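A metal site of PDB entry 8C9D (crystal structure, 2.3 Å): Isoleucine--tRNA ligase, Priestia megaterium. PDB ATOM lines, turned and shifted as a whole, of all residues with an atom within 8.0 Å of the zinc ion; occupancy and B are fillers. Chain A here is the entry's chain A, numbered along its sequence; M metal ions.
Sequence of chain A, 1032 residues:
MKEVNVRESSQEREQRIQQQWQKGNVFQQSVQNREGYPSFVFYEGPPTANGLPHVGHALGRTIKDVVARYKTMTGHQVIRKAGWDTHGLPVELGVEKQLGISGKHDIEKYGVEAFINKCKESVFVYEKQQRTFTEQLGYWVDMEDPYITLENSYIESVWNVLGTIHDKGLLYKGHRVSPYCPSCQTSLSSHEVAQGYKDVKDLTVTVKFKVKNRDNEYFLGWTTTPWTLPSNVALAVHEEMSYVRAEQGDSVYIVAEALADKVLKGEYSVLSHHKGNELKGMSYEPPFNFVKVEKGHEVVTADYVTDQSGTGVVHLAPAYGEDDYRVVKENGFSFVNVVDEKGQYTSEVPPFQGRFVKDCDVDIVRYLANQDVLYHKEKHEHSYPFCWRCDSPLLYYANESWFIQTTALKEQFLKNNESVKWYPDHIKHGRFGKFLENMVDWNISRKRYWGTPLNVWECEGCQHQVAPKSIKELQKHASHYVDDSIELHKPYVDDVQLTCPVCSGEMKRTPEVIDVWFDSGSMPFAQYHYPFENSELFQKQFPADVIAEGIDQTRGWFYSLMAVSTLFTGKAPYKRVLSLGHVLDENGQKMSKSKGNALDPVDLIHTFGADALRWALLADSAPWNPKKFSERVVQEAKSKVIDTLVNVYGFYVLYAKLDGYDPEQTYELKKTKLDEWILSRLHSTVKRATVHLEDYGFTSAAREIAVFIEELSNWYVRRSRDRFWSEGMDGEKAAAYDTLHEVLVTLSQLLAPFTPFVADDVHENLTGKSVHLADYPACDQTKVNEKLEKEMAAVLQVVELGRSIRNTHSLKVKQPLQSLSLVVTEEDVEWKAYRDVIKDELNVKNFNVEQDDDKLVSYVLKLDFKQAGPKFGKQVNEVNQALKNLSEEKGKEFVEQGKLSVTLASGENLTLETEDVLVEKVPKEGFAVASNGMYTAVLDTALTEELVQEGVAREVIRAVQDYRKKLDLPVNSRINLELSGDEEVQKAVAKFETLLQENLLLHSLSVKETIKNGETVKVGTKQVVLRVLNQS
O of Cys 184 sits at hydrogen-bond distance from NH1 of Arg 448 (3.0 Å). The backbone NH (N) of Ser 392 sits close to the side-chain sulfur (SG) of Cys 390 (3.3 Å). The backbone NH (N) of Arg 389 sits close to the side-chain sulfur (SG) of Cys 387 (3.5 Å). The backbone NH (N) of Cys 181 is in hydrogen-bond range of the backbone carbonyl oxygen (O) of Thr 186 (3.0 Å). The side-chain sulfur of Cys 181 lies close to the backbone NH of Ser 183 (3.6 Å). The backbone carbonyl oxygen (O) of Ser 392 lies within hydrogen-bond range of the backbone NH (N) of Cys 387 (2.8 Å).
Of the 20 residues printed, 4 come within 4 Å of the zinc ion. Along chain A the residues within 4 Å of the zinc ion span positions 181 to 390. The nearest printed residue that does not touch the zinc ion is Ser 183 (4.8 Å).
The zinc ion is bound by SG of Cys 181, 2.3 Å away. The zinc ion is bound by SG of Cys 184 (2.3 Å). The side-chain sulfur (SG) of Cys 387 is bound to the zinc ion (2.3 Å). The zinc ion is bound by the side-chain sulfur (SG) of Cys 390 (2.4 Å).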
ATOM      1  N   LEU A  89     -25.821  -9.894  26.859  1.00  0.00           N
ATOM      2  CA  LEU A  89     -24.907 -10.917  26.362  1.00  0.00           C
ATOM      3  C   LEU A  89     -24.375 -11.847  27.443  1.00  0.00           C
ATOM      4  O   LEU A  89     -24.274 -13.066  27.180  1.00  0.00           O
ATOM      5  CB  LEU A  89     -23.737 -10.251  25.620  1.00  0.00           C
ATOM      6  CG  LEU A  89     -24.101  -9.483  24.356  1.00  0.00           C
ATOM      7  CD1 LEU A  89     -23.023  -8.442  24.061  1.00  0.00           C
ATOM      8  CD2 LEU A  89     -24.251 -10.437  23.187  1.00  0.00           C
ATOM      9  N   LEU A  93     -25.245 -15.556  25.835  1.00  0.00           N
ATOM     10  CA  LEU A  93     -24.244 -16.464  25.270  1.00  0.00           C
ATOM     11  C   LEU A  93     -24.244 -17.803  25.999  1.00  0.00           C
ATOM     12  O   LEU A  93     -24.185 -18.869  25.363  1.00  0.00           O
ATOM     13  CB  LEU A  93     -22.866 -15.815  25.279  1.00  0.00           C
ATOM     14  CG  LEU A  93     -22.814 -14.530  24.448  1.00  0.00           C
ATOM     15  CD1 LEU A  93     -21.429 -13.902  24.446  1.00  0.00           C
ATOM     16  CD2 LEU A  93     -23.298 -14.781  23.029  1.00  0.00           C
ATOM     17  N   TYR A 180     -17.300  -3.258  17.134  1.00  0.00           N
ATOM     18  CA  TYR A 180     -18.326  -4.202  16.721  1.00  0.00           C
ATOM     19  C   TYR A 180     -17.783  -5.612  16.913  1.00  0.00           C
ATOM     20  O   TYR A 180     -16.638  -5.894  16.550  1.00  0.00           O
ATOM     21  CB  TYR A 180     -18.699  -3.954  15.257  1.00  0.00           C
ATOM     22  CG  TYR A 180     -19.811  -4.833  14.719  1.00  0.00           C
ATOM     23  CD1 TYR A 180     -21.141  -4.470  14.871  1.00  0.00           C
ATOM     24  CD2 TYR A 180     -19.522  -6.014  14.045  1.00  0.00           C
ATOM     25  CE1 TYR A 180     -22.160  -5.268  14.377  1.00  0.00           C
ATOM     26  CE2 TYR A 180     -20.533  -6.811  13.544  1.00  0.00           C
ATOM     27  CZ  TYR A 180     -21.845  -6.441  13.719  1.00  0.00           C
ATOM     28  OH  TYR A 180     -22.857  -7.238  13.219  1.00  0.00           O
ATOM     29  N   CYS A 181     -18.614  -6.480  17.481  1.00  0.00           N
ATOM     30  CA  CYS A 181     -18.264  -7.893  17.615  1.00  0.00           C
ATOM     31  C   CYS A 181     -18.820  -8.658  16.427  1.00  0.00           C
ATOM     32  O   CYS A 181     -20.056  -8.731  16.282  1.00  0.00           O
ATOM     33  CB  CYS A 181     -18.811  -8.486  18.895  1.00  0.00           C
ATOM     34  SG  CYS A 181     -18.291 -10.202  19.155  1.00  0.00           S
ATOM     35  N   PRO A 182     -17.980  -9.234  15.561  1.00  0.00           N
ATOM     36  CA  PRO A 182     -18.519  -9.997  14.424  1.00  0.00           C
ATOM     37  C   PRO A 182     -19.212 -11.292  14.829  1.00  0.00           C
ATOM     38  O   PRO A 182     -20.031 -11.802  14.054  1.00  0.00           O
ATOM     39  CB  PRO A 182     -17.265 -10.281  13.581  1.00  0.00           C
ATOM     40  CG  PRO A 182     -16.148 -10.262  14.563  1.00  0.00           C
ATOM     41  CD  PRO A 182     -16.511  -9.196  15.572  1.00  0.00           C
ATOM     42  N   SER A 183     -18.901 -11.848  15.999  1.00  0.00           N
ATOM     43  CA  SER A 183     -19.543 -13.079  16.474  1.00  0.00           C
ATOM     44  C   SER A 183     -20.871 -12.771  17.170  1.00  0.00           C
ATOM     45  O   SER A 183     -21.927 -13.285  16.768  1.00  0.00           O
ATOM     46  CB  SER A 183     -18.604 -13.837  17.411  1.00  0.00           C
ATOM     47  OG  SER A 183     -19.267 -14.941  18.006  1.00  0.00           O
ATOM     48  N   CYS A 184     -20.833 -11.935  18.217  1.00  0.00           N
ATOM     49  CA  CYS A 184     -22.068 -11.480  18.843  1.00  0.00           C
ATOM     50  C   CYS A 184     -22.929 -10.676  17.881  1.00  0.00           C
ATOM     51  O   CYS A 184     -24.146 -10.577  18.098  1.00  0.00           O
ATOM     52  CB  CYS A 184     -21.739 -10.649  20.083  1.00  0.00           C
ATOM     53  SG  CYS A 184     -20.952 -11.536  21.461  1.00  0.00           S
ATOM     54  N   GLN A 185     -22.333 -10.122  16.826  1.00  0.00           N
ATOM     55  CA  GLN A 185     -23.036  -9.363  15.781  1.00  0.00           C
ATOM     56  C   GLN A 185     -23.744  -8.144  16.351  1.00  0.00           C
ATOM     57  O   GLN A 185     -24.928  -7.897  16.097  1.00  0.00           O
ATOM     58  CB  GLN A 185     -23.998 -10.260  15.011  1.00  0.00           C
ATOM     59  CG  GLN A 185     -23.354 -11.450  14.322  1.00  0.00           C
ATOM     60  CD  GLN A 185     -24.339 -12.274  13.520  1.00  0.00           C
ATOM     61  OE1 GLN A 185     -25.233 -11.734  12.872  1.00  0.00           O
ATOM     62  NE2 GLN A 185     -24.188 -13.592  13.569  1.00  0.00           N
ATOM     63  N   THR A 186     -23.000  -7.341  17.127  1.00  0.00           N
ATOM     64  CA  THR A 186     -23.566  -6.129  17.694  1.00  0.00           C
ATOM     65  C   THR A 186     -22.438  -5.152  18.015  1.00  0.00           C
ATOM     66  O   THR A 186     -21.315  -5.552  18.316  1.00  0.00           O
ATOM     67  CB  THR A 186     -24.394  -6.419  18.948  1.00  0.00           C
ATOM     68  OG1 THR A 186     -25.036  -5.212  19.392  1.00  0.00           O
ATOM     69  CG2 THR A 186     -23.524  -6.970  20.068  1.00  0.00           C
ATOM     70  N   LEU A 188     -20.644  -2.305  20.448  1.00  0.00           N
ATOM     71  CA  LEU A 188     -20.344  -2.337  21.871  1.00  0.00           C
ATOM     72  C   LEU A 188     -20.004  -0.947  22.359  1.00  0.00           C
ATOM     73  O   LEU A 188     -19.600  -0.079  21.575  1.00  0.00           O
ATOM     74  CB  LEU A 188     -19.201  -3.302  22.189  1.00  0.00           C
ATOM     75  CG  LEU A 188     -19.463  -4.772  21.877  1.00  0.00           C
ATOM     76  CD1 LEU A 188     -18.180  -5.585  22.073  1.00  0.00           C
ATOM     77  CD2 LEU A 188     -20.600  -5.320  22.738  1.00  0.00           C
ATOM     78  N   PHE A 386     -10.718  -6.888  21.830  1.00  0.00           N
ATOM     79  CA  PHE A 386     -11.440  -8.157  21.749  1.00  0.00           C
ATOM     80  C   PHE A 386     -12.719  -8.057  22.582  1.00  0.00           C
ATOM     81  O   PHE A 386     -12.772  -7.303  23.571  1.00  0.00           O
ATOM     82  CB  PHE A 386     -10.558  -9.313  22.260  1.00  0.00           C
ATOM     83  CG  PHE A 386      -9.422  -9.681  21.326  1.00  0.00           C
ATOM     84  CD1 PHE A 386      -8.303  -8.870  21.235  1.00  0.00           C
ATOM     85  CD2 PHE A 386      -9.469 -10.831  20.565  1.00  0.00           C
ATOM     86  CE1 PHE A 386      -7.258  -9.196  20.385  1.00  0.00           C
ATOM     87  CE2 PHE A 386      -8.430 -11.167  19.723  1.00  0.00           C
ATOM     88  CZ  PHE A 386      -7.327 -10.351  19.630  1.00  0.00           C
ATOM     89  N   CYS A 387     -13.747  -8.824  22.177  1.00  0.00           N
ATOM     90  CA  CYS A 387     -15.033  -8.788  22.867  1.00  0.00           C
ATOM     91  C   CYS A 387     -14.913  -9.321  24.297  1.00  0.00           C
ATOM     92  O   CYS A 387     -14.428 -10.429  24.512  1.00  0.00           O
ATOM     93  CB  CYS A 387     -16.061  -9.597  22.094  1.00  0.00           C
ATOM     94  SG  CYS A 387     -17.701  -9.705  22.887  1.00  0.00           S
ATOM     95  N   TRP A 388     -15.398  -8.539  25.275  1.00  0.00           N
ATOM     96  CA  TRP A 388     -15.305  -8.873  26.686  1.00  0.00           C
ATOM     97  C   TRP A 388     -16.146 -10.094  27.065  1.00  0.00           C
ATOM     98  O   TRP A 388     -15.976 -10.629  28.180  1.00  0.00           O
ATOM     99  CB  TRP A 388     -15.706  -7.661  27.545  1.00  0.00           C
ATOM    100  CG  TRP A 388     -17.187  -7.377  27.552  1.00  0.00           C
ATOM    101  CD1 TRP A 388     -17.993  -7.094  26.485  1.00  0.00           C
ATOM    102  CD2 TRP A 388     -18.027  -7.383  28.707  1.00  0.00           C
ATOM    103  NE1 TRP A 388     -19.299  -6.915  26.904  1.00  0.00           N
ATOM    104  CE2 TRP A 388     -19.347  -7.083  28.266  1.00  0.00           C
ATOM    105  CE3 TRP A 388     -17.806  -7.600  30.070  1.00  0.00           C
ATOM    106  CZ2 TRP A 388     -20.426  -7.010  29.148  1.00  0.00           C
ATOM    107  CZ3 TRP A 388     -18.870  -7.525  30.939  1.00  0.00           C
ATOM    108  CH2 TRP A 388     -20.164  -7.232  30.480  1.00  0.00           C
ATOM    109  N   ARG A 389     -17.017 -10.560  26.171  1.00  0.00           N
ATOM    110  CA  ARG A 389     -17.741 -11.809  26.373  1.00  0.00           C
ATOM    111  C   ARG A 389     -17.316 -12.942  25.444  1.00  0.00           C
ATOM    112  O   ARG A 389     -16.906 -13.997  25.937  1.00  0.00           O
ATOM    113  CB  ARG A 389     -19.259 -11.592  26.262  1.00  0.00           C
ATOM    114  CG  ARG A 389     -19.793 -10.375  27.025  1.00  0.00           C
ATOM    115  CD  ARG A 389     -19.480 -10.425  28.523  1.00  0.00           C
ATOM    116  NE  ARG A 389     -19.865 -11.684  29.161  1.00  0.00           N
ATOM    117  CZ  ARG A 389     -19.689 -11.932  30.451  1.00  0.00           C
ATOM    118  NH1 ARG A 389     -19.155 -11.039  31.270  1.00  0.00           N
ATOM    119  NH2 ARG A 389     -20.069 -13.107  30.950  1.00  0.00           N
ATOM    120  N   CYS A 390     -17.411 -12.826  24.108  1.00  0.00           N
ATOM    121  CA  CYS A 390     -17.142 -14.029  23.311  1.00  0.00           C
ATOM    122  C   CYS A 390     -15.660 -14.265  23.062  1.00  0.00           C
ATOM    123  O   CYS A 390     -15.292 -15.321  22.547  1.00  0.00           O
ATOM    124  CB  CYS A 390     -17.804 -14.004  21.940  1.00  0.00           C
ATOM    125  SG  CYS A 390     -17.204 -12.769  20.850  1.00  0.00           S
ATOM    126  N   ASP A 391     -14.835 -13.243  23.278  1.00  0.00           N
ATOM    127  CA  ASP A 391     -13.395 -13.244  23.075  1.00  0.00           C
ATOM    128  C   ASP A 391     -12.992 -13.109  21.602  1.00  0.00           C
ATOM    129  O   ASP A 391     -11.800 -13.226  21.305  1.00  0.00           O
ATOM    130  CB  ASP A 391     -12.736 -14.505  23.665  1.00  0.00           C
ATOM    131  CG  ASP A 391     -11.536 -14.192  24.523  1.00  0.00           C
ATOM    132  OD1 ASP A 391     -10.663 -13.419  24.085  1.00  0.00           O
ATOM    133  OD2 ASP A 391     -11.482 -14.711  25.658  1.00  0.00           O
ATOM    134  N   SER A 392     -13.933 -12.891  20.677  1.00  0.00           N
ATOM    135  CA  SER A 392     -13.573 -12.649  19.294  1.00  0.00           C
ATOM    136  C   SER A 392     -12.839 -11.317  19.148  1.00  0.00           C
ATOM    137  O   SER A 392     -13.043 -10.399  19.949  1.00  0.00           O
ATOM    138  CB  SER A 392     -14.825 -12.634  18.421  1.00  0.00           C
ATOM    139  OG  SER A 392     -14.595 -11.989  17.176  1.00  0.00           O
ATOM    140  N   PRO A 393     -11.961 -11.196  18.148  1.00  0.00           N
ATOM    141  CA  PRO A 393     -11.434  -9.879  17.814  1.00  0.00           C
ATOM    142  C   PRO A 393     -12.555  -8.958  17.374  1.00  0.00           C
ATOM    143  O   PRO A 393     -13.494  -9.378  16.702  1.00  0.00           O
ATOM    144  CB  PRO A 393     -10.455 -10.159  16.672  1.00  0.00           C
ATOM    145  CG  PRO A 393     -10.908 -11.485  16.105  1.00  0.00           C
ATOM    146  CD  PRO A 393     -11.408 -12.256  17.290  1.00  0.00           C
ATOM    147  N   LEU A 394     -12.467  -7.694  17.775  1.00  0.00           N
ATOM    148  CA  LEU A 394     -13.450  -6.716  17.352  1.00  0.00           C
ATOM    149  C   LEU A 394     -13.056  -6.107  16.016  1.00  0.00           C
ATOM    150  O   LEU A 394     -11.922  -6.230  15.555  1.00  0.00           O
ATOM    151  CB  LEU A 394     -13.629  -5.610  18.400  1.00  0.00           C
ATOM    152  CG  LEU A 394     -14.079  -6.049  19.788  1.00  0.00           C
ATOM    153  CD1 LEU A 394     -14.309  -4.825  20.665  1.00  0.00           C
ATOM    154  CD2 LEU A 394     -15.328  -6.917  19.698  1.00  0.00           C
ATOM    155  N   ARG A 448     -29.837  -7.649  19.688  1.00  0.00           N
ATOM    156  CA  ARG A 448     -30.040  -8.904  20.404  1.00  0.00           C
ATOM    157  C   ARG A 448     -31.497  -9.053  20.830  1.00  0.00           C
ATOM    158  O   ARG A 448     -32.355  -8.274  20.402  1.00  0.00           O
ATOM    159  CB  ARG A 448     -29.113  -8.992  21.613  1.00  0.00           C
ATOM    160  CG  ARG A 448     -27.649  -8.764  21.301  1.00  0.00           C
ATOM    161  CD  ARG A 448     -27.067  -9.932  20.509  1.00  0.00           C
ATOM    162  NE  ARG A 448     -27.099 -11.182  21.260  1.00  0.00           N
ATOM    163  CZ  ARG A 448     -26.565 -12.318  20.838  1.00  0.00           C
ATOM    164  NH1 ARG A 448     -25.949 -12.400  19.666  1.00  0.00           N
ATOM    165  NH2 ARG A 448     -26.627 -13.397  21.608  1.00  0.00           N
HETATM  166 ZN    ZN M   1     -18.710 -11.008  21.263  1.00  0.00          ZN
